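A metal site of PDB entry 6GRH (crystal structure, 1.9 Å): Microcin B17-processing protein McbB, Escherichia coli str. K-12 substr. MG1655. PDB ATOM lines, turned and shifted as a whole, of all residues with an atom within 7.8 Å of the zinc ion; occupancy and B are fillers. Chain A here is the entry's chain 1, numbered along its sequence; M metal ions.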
ATOM      1  N   TYR A 157      12.001  11.489  20.268  1.00  0.00           N
ATOM      2  CA  TYR A 157      11.746  11.666  21.691  1.00  0.00           C
ATOM      3  C   TYR A 157      12.897  11.104  22.539  1.00  0.00           C
ATOM      4  O   TYR A 157      13.330  11.760  23.492  1.00  0.00           O
ATOM      5  CB  TYR A 157      10.416  11.042  22.111  1.00  0.00           C
ATOM      6  CG  TYR A 157       9.147  11.803  21.734  1.00  0.00           C
ATOM      7  CD1 TYR A 157       9.164  13.051  21.064  1.00  0.00           C
ATOM      8  CD2 TYR A 157       7.907  11.279  22.075  1.00  0.00           C
ATOM      9  CE1 TYR A 157       7.976  13.723  20.748  1.00  0.00           C
ATOM     10  CE2 TYR A 157       6.729  11.941  21.763  1.00  0.00           C
ATOM     11  CZ  TYR A 157       6.763  13.160  21.106  1.00  0.00           C
ATOM     12  OH  TYR A 157       5.573  13.803  20.847  1.00  0.00           O
ATOM     13  N   GLU A 161      14.080  14.444  24.443  1.00  0.00           N
ATOM     14  CA  GLU A 161      13.161  14.766  25.553  1.00  0.00           C
ATOM     15  C   GLU A 161      13.814  15.363  26.783  1.00  0.00           C
ATOM     16  O   GLU A 161      13.167  16.118  27.511  1.00  0.00           O
ATOM     17  CB  GLU A 161      12.397  13.525  26.049  1.00  0.00           C
ATOM     18  CG  GLU A 161      11.114  13.278  25.334  1.00  0.00           C
ATOM     19  CD  GLU A 161      10.333  12.106  25.909  1.00  0.00           C
ATOM     20  OE1 GLU A 161      10.885  11.267  26.665  1.00  0.00           O
ATOM     21  OE2 GLU A 161       9.151  12.014  25.607  1.00  0.00           O
ATOM     22  N   TYR A 184       4.082  19.472  22.445  1.00  0.00           N
ATOM     23  CA  TYR A 184       4.595  18.614  23.495  1.00  0.00           C
ATOM     24  C   TYR A 184       5.813  19.216  24.204  1.00  0.00           C
ATOM     25  O   TYR A 184       6.921  19.219  23.659  1.00  0.00           O
ATOM     26  CB  TYR A 184       4.943  17.237  22.916  1.00  0.00           C
ATOM     27  CG  TYR A 184       5.562  16.306  23.922  1.00  0.00           C
ATOM     28  CD1 TYR A 184       5.080  16.226  25.243  1.00  0.00           C
ATOM     29  CD2 TYR A 184       6.625  15.484  23.561  1.00  0.00           C
ATOM     30  CE1 TYR A 184       5.677  15.376  26.180  1.00  0.00           C
ATOM     31  CE2 TYR A 184       7.223  14.639  24.484  1.00  0.00           C
ATOM     32  CZ  TYR A 184       6.753  14.577  25.776  1.00  0.00           C
ATOM     33  OH  TYR A 184       7.392  13.732  26.633  1.00  0.00           O
ATOM     34  N   THR A 190       2.495  18.837  28.888  1.00  0.00           N
ATOM     35  CA  THR A 190       1.449  18.708  27.867  1.00  0.00           C
ATOM     36  C   THR A 190       1.542  17.356  27.125  1.00  0.00           C
ATOM     37  O   THR A 190       2.611  16.742  27.109  1.00  0.00           O
ATOM     38  CB  THR A 190       1.527  19.838  26.823  1.00  0.00           C
ATOM     39  OG1 THR A 190       2.808  19.858  26.225  1.00  0.00           O
ATOM     40  CG2 THR A 190       1.246  21.186  27.447  1.00  0.00           C
ATOM     41  N   PRO A 191       0.412  16.905  26.524  1.00  0.00           N
ATOM     42  CA  PRO A 191       0.394  15.583  25.878  1.00  0.00           C
ATOM     43  C   PRO A 191       1.270  15.470  24.663  1.00  0.00           C
ATOM     44  O   PRO A 191       1.356  16.381  23.870  1.00  0.00           O
ATOM     45  CB  PRO A 191      -1.083  15.404  25.474  1.00  0.00           C
ATOM     46  CG  PRO A 191      -1.844  16.303  26.380  1.00  0.00           C
ATOM     47  CD  PRO A 191      -0.941  17.493  26.553  1.00  0.00           C
ATOM     48  N   CYS A 192       1.860  14.281  24.524  1.00  0.00           N
ATOM     49  CA  CYS A 192       2.778  13.974  23.473  1.00  0.00           C
ATOM     50  C   CYS A 192       2.065  13.499  22.210  1.00  0.00           C
ATOM     51  O   CYS A 192       0.839  13.449  22.164  1.00  0.00           O
ATOM     52  CB  CYS A 192       3.741  12.913  24.008  1.00  0.00           C
ATOM     53  SG  CYS A 192       3.140  11.214  23.931  1.00  0.00           S
ATOM     54  N   HIS A 193       2.834  13.220  21.169  1.00  0.00           N
ATOM     55  CA  HIS A 193       2.286  12.675  19.927  1.00  0.00           C
ATOM     56  C   HIS A 193       1.392  11.452  20.097  1.00  0.00           C
ATOM     57  O   HIS A 193       0.357  11.329  19.435  1.00  0.00           O
ATOM     58  CB  HIS A 193       3.413  12.252  19.024  1.00  0.00           C
ATOM     59  CG  HIS A 193       2.957  11.477  17.851  1.00  0.00           C
ATOM     60  ND1 HIS A 193       2.210  12.031  16.840  1.00  0.00           N
ATOM     61  CD2 HIS A 193       3.153  10.177  17.513  1.00  0.00           C
ATOM     62  CE1 HIS A 193       1.956  11.096  15.935  1.00  0.00           C
ATOM     63  NE2 HIS A 193       2.527   9.967  16.317  1.00  0.00           N
ATOM     64  N   PHE A 194       1.804  10.524  20.949  1.00  0.00           N
ATOM     65  CA  PHE A 194       1.077   9.254  21.118  1.00  0.00           C
ATOM     66  C   PHE A 194      -0.286   9.510  21.778  1.00  0.00           C
ATOM     67  O   PHE A 194      -1.294   8.893  21.415  1.00  0.00           O
ATOM     68  CB  PHE A 194       1.967   8.206  21.791  1.00  0.00           C
ATOM     69  CG  PHE A 194       3.145   7.831  20.954  1.00  0.00           C
ATOM     70  CD1 PHE A 194       2.962   7.091  19.786  1.00  0.00           C
ATOM     71  CD2 PHE A 194       4.407   8.327  21.240  1.00  0.00           C
ATOM     72  CE1 PHE A 194       4.028   6.823  18.946  1.00  0.00           C
ATOM     73  CE2 PHE A 194       5.490   8.025  20.426  1.00  0.00           C
ATOM     74  CZ  PHE A 194       5.306   7.279  19.271  1.00  0.00           C
ATOM     75  N   CYS A 195      -0.338  10.508  22.668  1.00  0.00           N
ATOM     76  CA  CYS A 195      -1.611  10.980  23.188  1.00  0.00           C
ATOM     77  C   CYS A 195      -2.561  11.453  22.082  1.00  0.00           C
ATOM     78  O   CYS A 195      -3.775  11.199  22.149  1.00  0.00           O
ATOM     79  CB  CYS A 195      -1.409  12.083  24.237  1.00  0.00           C
ATOM     80  SG  CYS A 195      -0.627  11.514  25.759  1.00  0.00           S
ATOM     81  N   HIS A 196      -2.005  12.126  21.065  1.00  0.00           N
ATOM     82  CA  HIS A 196      -2.770  12.650  19.935  1.00  0.00           C
ATOM     83  C   HIS A 196      -3.245  11.562  18.991  1.00  0.00           C
ATOM     84  O   HIS A 196      -4.477  11.469  18.678  1.00  0.00           O
ATOM     85  CB  HIS A 196      -1.971  13.726  19.174  1.00  0.00           C
ATOM     86  CG  HIS A 196      -1.917  15.024  19.896  1.00  0.00           C
ATOM     87  ND1 HIS A 196      -1.044  15.263  20.934  1.00  0.00           N
ATOM     88  CD2 HIS A 196      -2.687  16.137  19.784  1.00  0.00           C
ATOM     89  CE1 HIS A 196      -1.240  16.478  21.398  1.00  0.00           C
ATOM     90  NE2 HIS A 196      -2.236  17.030  20.729  1.00  0.00           N
ATOM     91  N   ILE A 285      -6.650  15.155  25.598  1.00  0.00           N
ATOM     92  CA  ILE A 285      -6.247  14.679  26.916  1.00  0.00           C
ATOM     93  C   ILE A 285      -5.037  13.750  26.810  1.00  0.00           C
ATOM     94  O   ILE A 285      -4.716  13.231  25.737  1.00  0.00           O
ATOM     95  CB  ILE A 285      -7.410  13.980  27.664  1.00  0.00           C
ATOM     96  CG1 ILE A 285      -7.874  12.706  26.967  1.00  0.00           C
ATOM     97  CG2 ILE A 285      -8.599  14.928  27.816  1.00  0.00           C
ATOM     98  CD1 ILE A 285      -8.829  11.863  27.779  1.00  0.00           C
ATOM     99  N   HIS A 286      -4.336  13.586  27.921  1.00  0.00           N
ATOM    100  CA  HIS A 286      -3.301  12.535  28.025  1.00  0.00           C
ATOM    101  C   HIS A 286      -3.966  11.171  27.851  1.00  0.00           C
ATOM    102  O   HIS A 286      -5.041  10.923  28.397  1.00  0.00           O
ATOM    103  CB  HIS A 286      -2.622  12.576  29.394  1.00  0.00           C
ATOM    104  CG  HIS A 286      -1.759  13.776  29.606  1.00  0.00           C
ATOM    105  ND1 HIS A 286      -2.249  14.960  30.120  1.00  0.00           N
ATOM    106  CD2 HIS A 286      -0.445  13.971  29.379  1.00  0.00           C
ATOM    107  CE1 HIS A 286      -1.255  15.834  30.193  1.00  0.00           C
ATOM    108  NE2 HIS A 286      -0.152  15.258  29.754  1.00  0.00           N
ATOM    109  N   TRP A 287      -3.363  10.324  27.033  1.00  0.00           N
ATOM    110  CA  TRP A 287      -3.914   8.999  26.820  1.00  0.00           C
ATOM    111  C   TRP A 287      -3.586   8.156  28.062  1.00  0.00           C
ATOM    112  O   TRP A 287      -2.453   8.193  28.575  1.00  0.00           O
ATOM    113  CB  TRP A 287      -3.354   8.389  25.566  1.00  0.00           C
ATOM    114  CG  TRP A 287      -3.806   7.015  25.287  1.00  0.00           C
ATOM    115  CD1 TRP A 287      -5.067   6.526  25.382  1.00  0.00           C
ATOM    116  CD2 TRP A 287      -2.996   5.961  24.779  1.00  0.00           C
ATOM    117  NE1 TRP A 287      -5.099   5.231  24.966  1.00  0.00           N
ATOM    118  CE2 TRP A 287      -3.832   4.853  24.580  1.00  0.00           C
ATOM    119  CE3 TRP A 287      -1.631   5.852  24.447  1.00  0.00           C
ATOM    120  CZ2 TRP A 287      -3.355   3.643  24.079  1.00  0.00           C
ATOM    121  CZ3 TRP A 287      -1.153   4.646  23.955  1.00  0.00           C
ATOM    122  CH2 TRP A 287      -2.020   3.548  23.774  1.00  0.00           C
ATOM    123  N   GLN A 288      -4.591   7.469  28.573  1.00  0.00           N
ATOM    124  CA  GLN A 288      -4.440   6.670  29.786  1.00  0.00           C
ATOM    125  C   GLN A 288      -3.266   5.678  29.753  1.00  0.00           C
ATOM    126  O   GLN A 288      -2.671   5.420  30.807  1.00  0.00           O
ATOM    127  CB  GLN A 288      -5.736   5.926  30.139  1.00  0.00           C
ATOM    128  CG  GLN A 288      -6.238   4.970  29.069  1.00  0.00           C
ATOM    129  CD  GLN A 288      -7.642   4.506  29.340  1.00  0.00           C
ATOM    130  OE1 GLN A 288      -8.089   4.434  30.493  1.00  0.00           O
ATOM    131  NE2 GLN A 288      -8.386   4.232  28.273  1.00  0.00           N
ATOM    132  N   ALA A 289      -2.998   5.085  28.581  1.00  0.00           N
ATOM    133  CA  ALA A 289      -1.920   4.122  28.448  1.00  0.00           C
ATOM    134  C   ALA A 289      -0.574   4.704  28.036  1.00  0.00           C
ATOM    135  O   ALA A 289       0.349   3.926  27.820  1.00  0.00           O
ATOM    136  CB  ALA A 289      -2.285   3.013  27.479  1.00  0.00           C
ATOM    137  N   CYS A 290      -0.456   6.024  27.936  1.00  0.00           N
ATOM    138  CA  CYS A 290       0.793   6.657  27.546  1.00  0.00           C
ATOM    139  C   CYS A 290       1.672   6.906  28.755  1.00  0.00           C
ATOM    140  O   CYS A 290       1.191   7.291  29.791  1.00  0.00           O
ATOM    141  CB  CYS A 290       0.535   7.988  26.863  1.00  0.00           C
ATOM    142  SG  CYS A 290       1.997   8.625  26.009  1.00  0.00           S
ATOM    143  N   SER A 291       2.971   6.786  28.582  1.00  0.00           N
ATOM    144  CA  SER A 291       3.925   7.054  29.672  1.00  0.00           C
ATOM    145  C   SER A 291       4.608   8.435  29.596  1.00  0.00           C
ATOM    146  O   SER A 291       5.528   8.682  30.390  1.00  0.00           O
ATOM    147  CB  SER A 291       4.982   5.972  29.614  1.00  0.00           C
ATOM    148  OG  SER A 291       5.540   6.010  28.311  1.00  0.00           O
ATOM    149  N   CYS A 292       4.164   9.339  28.711  1.00  0.00           N
ATOM    150  CA  CYS A 292       4.823  10.657  28.609  1.00  0.00           C
ATOM    151  C   CYS A 292       4.845  11.443  29.923  1.00  0.00           C
ATOM    152  O   CYS A 292       5.825  12.086  30.264  1.00  0.00           O
ATOM    153  CB  CYS A 292       4.263  11.521  27.469  1.00  0.00           C
ATOM    154  SG  CYS A 292       2.505  11.926  27.528  1.00  0.00           S
ATOM    155  N   LEU A 293       3.756  11.353  30.671  1.00  0.00           N
ATOM    156  CA  LEU A 293       3.618  11.998  31.983  1.00  0.00           C
ATOM    157  C   LEU A 293       4.598  11.507  33.030  1.00  0.00           C
ATOM    158  O   LEU A 293       4.948  12.246  33.957  1.00  0.00           O
ATOM    159  CB  LEU A 293       2.230  11.727  32.540  1.00  0.00           C
ATOM    160  CG  LEU A 293       1.165  12.583  31.900  1.00  0.00           C
ATOM    161  CD1 LEU A 293      -0.193  12.151  32.398  1.00  0.00           C
ATOM    162  CD2 LEU A 293       1.462  14.043  32.218  1.00  0.00           C
ATOM    163  N   ARG A 295       7.677  10.318  32.449  1.00  0.00           N
ATOM    164  CA  ARG A 295       9.086  10.551  32.127  1.00  0.00           C
ATOM    165  C   ARG A 295       9.643  11.831  32.755  1.00  0.00           C
ATOM    166  O   ARG A 295       8.920  12.774  33.082  1.00  0.00           O
ATOM    167  CB  ARG A 295       9.313  10.497  30.605  1.00  0.00           C
ATOM    168  CG  ARG A 295       9.125   9.083  30.067  1.00  0.00           C
ATOM    169  CD  ARG A 295       9.870   8.794  28.779  1.00  0.00           C
ATOM    170  NE  ARG A 295       9.248   9.505  27.674  1.00  0.00           N
ATOM    171  CZ  ARG A 295       8.134   9.122  27.031  1.00  0.00           C
ATOM    172  NH1 ARG A 295       7.474   8.019  27.365  1.00  0.00           N
ATOM    173  NH2 ARG A 295       7.673   9.871  26.018  1.00  0.00           N
ATOM    174  OXT ARG A 295      10.848  11.941  33.005  1.00  0.00           O
HETATM  175 ZN    ZN M   1       1.616  10.875  25.659  1.00  0.00          ZN
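The side-chain sulfur (SG) of Cys 290 binds the zinc ion (2.3 Å).
The side-chain sulfur (SG) of Cys 292 is bound to the zinc ion (2.3 Å).
SG of Cys 192 binds the zinc ion, 2.3 Å away.
The zinc ion is bound by the side-chain sulfur (SG) of Cys 195 (2.3 Å).
Of the 20 residues printed, 4 come within 4 Å of the zinc ion.
Along chain A the residues within 4 Å of the zinc ion span positions 192 to 292.
The nearest printed residue that does not touch the zinc ion is Phe 194 (4.5 Å).
The backbone NH of Trp 287 lies close to the side-chain sulfur of Cys 195.
O of Cys 192 sits at hydrogen-bond distance from ND1 of His 196, at 2.9 Å.
The backbone NH of Phe 194 sits close to the side-chain sulfur of Cys 192, 3.3 Å away.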
